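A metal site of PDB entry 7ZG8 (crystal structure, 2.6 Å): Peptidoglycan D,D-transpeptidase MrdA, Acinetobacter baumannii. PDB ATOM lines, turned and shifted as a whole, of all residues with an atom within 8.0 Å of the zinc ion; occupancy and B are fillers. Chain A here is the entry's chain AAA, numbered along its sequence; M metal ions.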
ATOM      1  N   ILE A 318      16.139  10.379 -26.057  1.00  0.00           N
ATOM      2  CA  ILE A 318      15.281  11.063 -27.065  1.00  0.00           C
ATOM      3  C   ILE A 318      15.443  12.579 -26.893  1.00  0.00           C
ATOM      4  O   ILE A 318      15.534  13.049 -25.732  1.00  0.00           O
ATOM      5  CB  ILE A 318      13.810  10.599 -26.985  1.00  0.00           C
ATOM      6  CG1 ILE A 318      13.135  10.949 -25.660  1.00  0.00           C
ATOM      7  CG2 ILE A 318      13.690   9.113 -27.296  1.00  0.00           C
ATOM      8  CD1 ILE A 318      12.262  12.170 -25.708  1.00  0.00           C
ATOM      9  N   SER A 319      15.515  13.306 -28.018  1.00  0.00           N
ATOM     10  CA  SER A 319      15.317  14.772 -28.056  1.00  0.00           C
ATOM     11  C   SER A 319      13.868  15.054 -27.658  1.00  0.00           C
ATOM     12  O   SER A 319      12.976  14.524 -28.350  1.00  0.00           O
ATOM     13  CB  SER A 319      15.646  15.374 -29.400  1.00  0.00           C
ATOM     14  OG  SER A 319      16.889  16.055 -29.346  1.00  0.00           O
ATOM     15  N   ASP A 320      13.664  15.793 -26.563  1.00  0.00           N
ATOM     16  CA  ASP A 320      12.317  16.144 -26.045  1.00  0.00           C
ATOM     17  C   ASP A 320      12.059  17.610 -26.354  1.00  0.00           C
ATOM     18  O   ASP A 320      12.505  18.485 -25.597  1.00  0.00           O
ATOM     19  CB  ASP A 320      12.174  15.849 -24.548  1.00  0.00           C
ATOM     20  CG  ASP A 320      10.757  16.000 -24.003  1.00  0.00           C
ATOM     21  OD1 ASP A 320       9.808  16.155 -24.783  1.00  0.00           O
ATOM     22  OD2 ASP A 320      10.638  15.978 -22.790  1.00  0.00           O
ATOM     23  N   PRO A 321      11.313  17.921 -27.449  1.00  0.00           N
ATOM     24  CA  PRO A 321      10.896  19.296 -27.737  1.00  0.00           C
ATOM     25  C   PRO A 321       9.643  19.723 -26.946  1.00  0.00           C
ATOM     26  O   PRO A 321       9.234  20.860 -27.131  1.00  0.00           O
ATOM     27  CB  PRO A 321      10.615  19.229 -29.237  1.00  0.00           C
ATOM     28  CG  PRO A 321      10.025  17.844 -29.427  1.00  0.00           C
ATOM     29  CD  PRO A 321      10.753  16.970 -28.432  1.00  0.00           C
ATOM     30  N   GLY A 322       9.088  18.836 -26.095  1.00  0.00           N
ATOM     31  CA  GLY A 322       7.879  19.068 -25.284  1.00  0.00           C
ATOM     32  C   GLY A 322       6.623  18.618 -26.001  1.00  0.00           C
ATOM     33  O   GLY A 322       5.527  18.982 -25.529  1.00  0.00           O
ATOM     34  N   TYR A 323       6.768  17.841 -27.089  1.00  0.00           N
ATOM     35  CA  TYR A 323       5.622  17.282 -27.869  1.00  0.00           C
ATOM     36  C   TYR A 323       6.100  16.097 -28.716  1.00  0.00           C
ATOM     37  O   TYR A 323       7.340  15.868 -28.878  1.00  0.00           O
ATOM     38  CB  TYR A 323       4.951  18.351 -28.744  1.00  0.00           C
ATOM     39  CG  TYR A 323       5.875  19.179 -29.600  1.00  0.00           C
ATOM     40  CD1 TYR A 323       6.344  18.713 -30.828  1.00  0.00           C
ATOM     41  CD2 TYR A 323       6.263  20.453 -29.214  1.00  0.00           C
ATOM     42  CE1 TYR A 323       7.188  19.472 -31.622  1.00  0.00           C
ATOM     43  CE2 TYR A 323       7.098  21.231 -30.000  1.00  0.00           C
ATOM     44  CZ  TYR A 323       7.560  20.735 -31.211  1.00  0.00           C
ATOM     45  OH  TYR A 323       8.386  21.502 -31.980  1.00  0.00           O
ATOM     46  N   ARG A 334       1.051  16.771 -26.435  1.00  0.00           N
ATOM     47  CA  ARG A 334       1.921  17.676 -25.644  1.00  0.00           C
ATOM     48  C   ARG A 334       2.478  16.929 -24.432  1.00  0.00           C
ATOM     49  O   ARG A 334       1.765  16.120 -23.818  1.00  0.00           O
ATOM     50  CB  ARG A 334       1.148  18.940 -25.260  1.00  0.00           C
ATOM     51  CG  ARG A 334       0.739  19.809 -26.450  1.00  0.00           C
ATOM     52  CD  ARG A 334       1.887  20.566 -27.097  1.00  0.00           C
ATOM     53  NE  ARG A 334       1.636  21.015 -28.467  1.00  0.00           N
ATOM     54  CZ  ARG A 334       2.468  21.774 -29.208  1.00  0.00           C
ATOM     55  NH1 ARG A 334       3.632  22.201 -28.724  1.00  0.00           N
ATOM     56  NH2 ARG A 334       2.136  22.117 -30.432  1.00  0.00           N
ATOM     57  N   ASP A 335       3.731  17.220 -24.100  1.00  0.00           N
ATOM     58  CA  ASP A 335       4.372  16.791 -22.840  1.00  0.00           C
ATOM     59  C   ASP A 335       3.734  17.612 -21.721  1.00  0.00           C
ATOM     60  O   ASP A 335       3.297  18.751 -22.010  1.00  0.00           O
ATOM     61  CB  ASP A 335       5.893  16.937 -22.950  1.00  0.00           C
ATOM     62  CG  ASP A 335       6.690  16.070 -22.004  1.00  0.00           C
ATOM     63  OD1 ASP A 335       6.220  15.823 -20.884  1.00  0.00           O
ATOM     64  OD2 ASP A 335       7.758  15.624 -22.414  1.00  0.00           O
ATOM     65  N   TRP A 336       3.628  17.056 -20.501  1.00  0.00           N
ATOM     66  CA  TRP A 336       3.070  17.780 -19.333  1.00  0.00           C
ATOM     67  C   TRP A 336       3.815  19.114 -19.161  1.00  0.00           C
ATOM     68  O   TRP A 336       3.143  20.080 -18.760  1.00  0.00           O
ATOM     69  CB  TRP A 336       3.044  16.935 -18.050  1.00  0.00           C
ATOM     70  CG  TRP A 336       4.374  16.602 -17.442  1.00  0.00           C
ATOM     71  CD1 TRP A 336       5.077  15.448 -17.627  1.00  0.00           C
ATOM     72  CD2 TRP A 336       5.146  17.398 -16.517  1.00  0.00           C
ATOM     73  NE1 TRP A 336       6.237  15.481 -16.899  1.00  0.00           N
ATOM     74  CE2 TRP A 336       6.316  16.665 -16.219  1.00  0.00           C
ATOM     75  CE3 TRP A 336       4.967  18.654 -15.924  1.00  0.00           C
ATOM     76  CZ2 TRP A 336       7.305  17.156 -15.355  1.00  0.00           C
ATOM     77  CZ3 TRP A 336       5.935  19.131 -15.063  1.00  0.00           C
ATOM     78  CH2 TRP A 336       7.086  18.394 -14.790  1.00  0.00           C
ATOM     79  N   LYS A 337       5.115  19.149 -19.476  1.00  0.00           N
ATOM     80  CA  LYS A 337       5.985  20.360 -19.527  1.00  0.00           C
ATOM     81  C   LYS A 337       6.327  20.684 -20.997  1.00  0.00           C
ATOM     82  O   LYS A 337       7.102  19.916 -21.597  1.00  0.00           O
ATOM     83  CB  LYS A 337       7.227  20.106 -18.686  1.00  0.00           C
ATOM     84  CG  LYS A 337       8.212  21.249 -18.567  1.00  0.00           C
ATOM     85  CD  LYS A 337       9.164  21.041 -17.387  1.00  0.00           C
ATOM     86  CE  LYS A 337      10.301  22.043 -17.292  1.00  0.00           C
ATOM     87  NZ  LYS A 337      11.369  21.772 -18.299  1.00  0.00           N
ATOM     88  N   LYS A 338       5.793  21.787 -21.547  1.00  0.00           N
ATOM     89  CA  LYS A 338       5.746  22.027 -23.018  1.00  0.00           C
ATOM     90  C   LYS A 338       7.095  22.545 -23.541  1.00  0.00           C
ATOM     91  O   LYS A 338       7.265  22.533 -24.769  1.00  0.00           O
ATOM     92  CB  LYS A 338       4.551  22.904 -23.423  1.00  0.00           C
ATOM     93  CG  LYS A 338       3.291  22.098 -23.724  1.00  0.00           C
ATOM     94  CD  LYS A 338       1.974  22.865 -23.709  1.00  0.00           C
ATOM     95  CE  LYS A 338       0.809  22.072 -23.135  1.00  0.00           C
ATOM     96  NZ  LYS A 338      -0.344  22.948 -22.798  1.00  0.00           N
ATOM     97  N   THR A 339       8.026  22.947 -22.661  1.00  0.00           N
ATOM     98  CA  THR A 339       9.469  23.122 -23.004  1.00  0.00           C
ATOM     99  C   THR A 339      10.169  21.766 -23.188  1.00  0.00           C
ATOM    100  O   THR A 339      11.217  21.741 -23.833  1.00  0.00           O
ATOM    101  CB  THR A 339      10.247  23.906 -21.942  1.00  0.00           C
ATOM    102  OG1 THR A 339      10.035  23.308 -20.663  1.00  0.00           O
ATOM    103  CG2 THR A 339       9.855  25.369 -21.894  1.00  0.00           C
ATOM    104  N   GLY A 340       9.646  20.689 -22.604  1.00  0.00           N
ATOM    105  CA  GLY A 340      10.283  19.352 -22.612  1.00  0.00           C
ATOM    106  C   GLY A 340      11.319  19.213 -21.517  1.00  0.00           C
ATOM    107  O   GLY A 340      11.445  20.129 -20.661  1.00  0.00           O
ATOM    108  N   HIS A 341      12.021  18.078 -21.508  1.00  0.00           N
ATOM    109  CA  HIS A 341      12.987  17.643 -20.487  1.00  0.00           C
ATOM    110  C   HIS A 341      14.389  17.486 -21.116  1.00  0.00           C
ATOM    111  O   HIS A 341      15.292  16.915 -20.435  1.00  0.00           O
ATOM    112  CB  HIS A 341      12.444  16.363 -19.842  1.00  0.00           C
ATOM    113  CG  HIS A 341      11.202  16.590 -19.052  1.00  0.00           C
ATOM    114  ND1 HIS A 341       9.922  16.359 -19.557  1.00  0.00           N
ATOM    115  CD2 HIS A 341      11.038  17.049 -17.787  1.00  0.00           C
ATOM    116  CE1 HIS A 341       9.039  16.652 -18.630  1.00  0.00           C
ATOM    117  NE2 HIS A 341       9.697  17.076 -17.534  1.00  0.00           N
ATOM    118  N   GLY A 342      14.579  17.992 -22.340  1.00  0.00           N
ATOM    119  CA  GLY A 342      15.874  17.968 -23.060  1.00  0.00           C
ATOM    120  C   GLY A 342      16.184  16.600 -23.654  1.00  0.00           C
ATOM    121  O   GLY A 342      15.359  16.094 -24.468  1.00  0.00           O
ATOM    122  N   VAL A 344      16.426  12.845 -22.949  1.00  0.00           N
ATOM    123  CA  VAL A 344      15.647  12.033 -21.969  1.00  0.00           C
ATOM    124  C   VAL A 344      15.915  10.543 -22.222  1.00  0.00           C
ATOM    125  O   VAL A 344      15.473  10.039 -23.273  1.00  0.00           O
ATOM    126  CB  VAL A 344      14.141  12.355 -22.067  1.00  0.00           C
ATOM    127  CG1 VAL A 344      13.322  11.601 -21.027  1.00  0.00           C
ATOM    128  CG2 VAL A 344      13.862  13.846 -21.978  1.00  0.00           C
ATOM    129  N   LYS A 348      15.580   9.212 -16.674  1.00  0.00           N
ATOM    130  CA  LYS A 348      15.086  10.620 -16.662  1.00  0.00           C
ATOM    131  C   LYS A 348      13.563  10.610 -16.885  1.00  0.00           C
ATOM    132  O   LYS A 348      12.854  11.333 -16.157  1.00  0.00           O
ATOM    133  CB  LYS A 348      15.797  11.501 -17.685  1.00  0.00           C
ATOM    134  CG  LYS A 348      15.971  12.959 -17.265  1.00  0.00           C
ATOM    135  CD  LYS A 348      16.617  13.829 -18.333  1.00  0.00           C
ATOM    136  CE  LYS A 348      16.959  15.204 -17.816  1.00  0.00           C
ATOM    137  NZ  LYS A 348      17.624  16.028 -18.848  1.00  0.00           N
ATOM    138  N   ALA A 349      13.074   9.791 -17.825  1.00  0.00           N
ATOM    139  CA  ALA A 349      11.626   9.687 -18.135  1.00  0.00           C
ATOM    140  C   ALA A 349      10.828   9.320 -16.881  1.00  0.00           C
ATOM    141  O   ALA A 349       9.744   9.893 -16.729  1.00  0.00           O
ATOM    142  CB  ALA A 349      11.424   8.688 -19.252  1.00  0.00           C
ATOM    143  N   MET A 352      11.261  12.347 -13.875  1.00  0.00           N
ATOM    144  CA  MET A 352      10.591  13.585 -14.366  1.00  0.00           C
ATOM    145  C   MET A 352       9.265  13.277 -15.087  1.00  0.00           C
ATOM    146  O   MET A 352       8.668  14.243 -15.565  1.00  0.00           O
ATOM    147  CB  MET A 352      11.522  14.391 -15.279  1.00  0.00           C
ATOM    148  CG  MET A 352      12.513  15.252 -14.492  1.00  0.00           C
ATOM    149  SD  MET A 352      13.846  15.866 -15.517  1.00  0.00           S
ATOM    150  CE  MET A 352      15.093  16.177 -14.269  1.00  0.00           C
ATOM    151  N   SER A 353       8.809  12.029 -15.130  1.00  0.00           N
ATOM    152  CA  SER A 353       7.478  11.618 -15.641  1.00  0.00           C
ATOM    153  C   SER A 353       7.301  12.011 -17.121  1.00  0.00           C
ATOM    154  O   SER A 353       6.152  12.318 -17.523  1.00  0.00           O
ATOM    155  CB  SER A 353       6.378  12.191 -14.788  1.00  0.00           C
ATOM    156  OG  SER A 353       5.155  11.535 -15.020  1.00  0.00           O
ATOM    157  N   CYS A 354       8.390  12.016 -17.906  1.00  0.00           N
ATOM    158  CA  CYS A 354       8.420  12.595 -19.272  1.00  0.00           C
ATOM    159  C   CYS A 354       7.397  11.886 -20.158  1.00  0.00           C
ATOM    160  O   CYS A 354       7.591  10.710 -20.398  1.00  0.00           O
ATOM    161  CB  CYS A 354       9.804  12.506 -19.910  1.00  0.00           C
ATOM    162  SG  CYS A 354       9.740  13.159 -21.566  1.00  0.00           S
ATOM    163  N   ASP A 355       6.349  12.579 -20.605  1.00  0.00           N
ATOM    164  CA  ASP A 355       5.312  12.010 -21.505  1.00  0.00           C
ATOM    165  C   ASP A 355       5.885  11.733 -22.895  1.00  0.00           C
ATOM    166  O   ASP A 355       5.349  10.840 -23.569  1.00  0.00           O
ATOM    167  CB  ASP A 355       4.109  12.937 -21.659  1.00  0.00           C
ATOM    168  CG  ASP A 355       3.314  13.127 -20.387  1.00  0.00           C
ATOM    169  OD1 ASP A 355       3.395  12.237 -19.517  1.00  0.00           O
ATOM    170  OD2 ASP A 355       2.634  14.159 -20.278  1.00  0.00           O
ATOM    171  N   THR A 356       6.901  12.471 -23.344  1.00  0.00           N
ATOM    172  CA  THR A 356       7.397  12.385 -24.741  1.00  0.00           C
ATOM    173  C   THR A 356       8.072  11.025 -24.942  1.00  0.00           C
ATOM    174  O   THR A 356       7.712  10.334 -25.922  1.00  0.00           O
ATOM    175  CB  THR A 356       8.290  13.585 -25.092  1.00  0.00           C
ATOM    176  OG1 THR A 356       7.633  14.803 -24.740  1.00  0.00           O
ATOM    177  CG2 THR A 356       8.643  13.648 -26.567  1.00  0.00           C
ATOM    178  N   TYR A 357       8.986  10.648 -24.038  1.00  0.00           N
ATOM    179  CA  TYR A 357       9.680   9.331 -24.007  1.00  0.00           C
ATOM    180  C   TYR A 357       8.697   8.181 -24.270  1.00  0.00           C
ATOM    181  O   TYR A 357       9.026   7.271 -25.059  1.00  0.00           O
ATOM    182  CB  TYR A 357      10.370   9.104 -22.655  1.00  0.00           C
ATOM    183  CG  TYR A 357      11.251   7.885 -22.601  1.00  0.00           C
ATOM    184  CD1 TYR A 357      10.743   6.635 -22.318  1.00  0.00           C
ATOM    185  CD2 TYR A 357      12.614   8.004 -22.832  1.00  0.00           C
ATOM    186  CE1 TYR A 357      11.562   5.519 -22.252  1.00  0.00           C
ATOM    187  CE2 TYR A 357      13.446   6.900 -22.769  1.00  0.00           C
ATOM    188  CZ  TYR A 357      12.924   5.647 -22.483  1.00  0.00           C
ATOM    189  OH  TYR A 357      13.768   4.574 -22.447  1.00  0.00           O
ATOM    190  N   PHE A 358       7.543   8.223 -23.600  1.00  0.00           N
ATOM    191  CA  PHE A 358       6.519   7.152 -23.573  1.00  0.00           C
ATOM    192  C   PHE A 358       5.635   7.235 -24.821  1.00  0.00           C
ATOM    193  O   PHE A 358       5.194   6.183 -25.256  1.00  0.00           O
ATOM    194  CB  PHE A 358       5.762   7.147 -22.236  1.00  0.00           C
ATOM    195  CG  PHE A 358       6.634   6.654 -21.101  1.00  0.00           C
ATOM    196  CD1 PHE A 358       6.886   5.301 -20.935  1.00  0.00           C
ATOM    197  CD2 PHE A 358       7.245   7.546 -20.231  1.00  0.00           C
ATOM    198  CE1 PHE A 358       7.708   4.856 -19.916  1.00  0.00           C
ATOM    199  CE2 PHE A 358       8.061   7.100 -19.204  1.00  0.00           C
ATOM    200  CZ  PHE A 358       8.297   5.745 -19.050  1.00  0.00           C
ATOM    201  N   TYR A 359       5.402   8.430 -25.368  1.00  0.00           N
ATOM    202  CA  TYR A 359       4.693   8.606 -26.662  1.00  0.00           C
ATOM    203  C   TYR A 359       5.509   7.942 -27.774  1.00  0.00           C
ATOM    204  O   TYR A 359       4.889   7.271 -28.614  1.00  0.00           O
ATOM    205  CB  TYR A 359       4.528  10.071 -27.053  1.00  0.00           C
ATOM    206  CG  TYR A 359       3.665  10.931 -26.170  1.00  0.00           C
ATOM    207  CD1 TYR A 359       2.569  10.436 -25.486  1.00  0.00           C
ATOM    208  CD2 TYR A 359       3.923  12.286 -26.062  1.00  0.00           C
ATOM    209  CE1 TYR A 359       1.751  11.256 -24.731  1.00  0.00           C
ATOM    210  CE2 TYR A 359       3.128  13.120 -25.290  1.00  0.00           C
ATOM    211  CZ  TYR A 359       2.030  12.603 -24.633  1.00  0.00           C
ATOM    212  OH  TYR A 359       1.251  13.429 -23.863  1.00  0.00           O
HETATM  213 ZN    ZN M   1       9.403  15.476 -21.366  1.00  0.00          ZN
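The zinc ion is bound by the side-chain carboxylate of Asp 320 (2.0 Å), the side-chain carboxylate of Asp 335 (2.0 Å), a ring nitrogen (ND1) of His 341 (2.1 Å) and the side-chain sulfur of Cys 354 (2.3 Å). The zinc ion has four donor atoms within binding distance.
The side-chain hydroxyl (OG1) of Thr 356 sits at hydrogen-bond distance from the side-chain carboxylate (OD1) of Asp 320. N of Gly 322 is in hydrogen-bond range of OD1 of Asp 320 (3.1 Å). The backbone NH of Asp 320 sits at hydrogen-bond distance from the backbone carbonyl oxygen of Gly 342 (2.7 Å). OD2 of Asp 335 sits close to OG1 of Thr 356, 2.5 Å away. The backbone NH (N) of Asp 355 lies within hydrogen-bond range of the side-chain carboxylate (OD1) of Asp 335 (3.3 Å). The backbone NH (N) of Asp 335 sits at hydrogen-bond distance from the backbone carbonyl oxygen (O) of Gly 322 (2.9 Å). O of His 341 is in hydrogen-bond range of NZ of Lys 348, at 3.0 Å. The side-chain sulfur of Cys 354 sits close to the backbone NH of Thr 356 (3.4 Å).
Thr 356 touches the zinc ion. Of the 26 residues printed, 5 come within 4 Å of the zinc ion. The nearest printed residue that does not touch the zinc ion is Gly 340 (4.2 Å).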
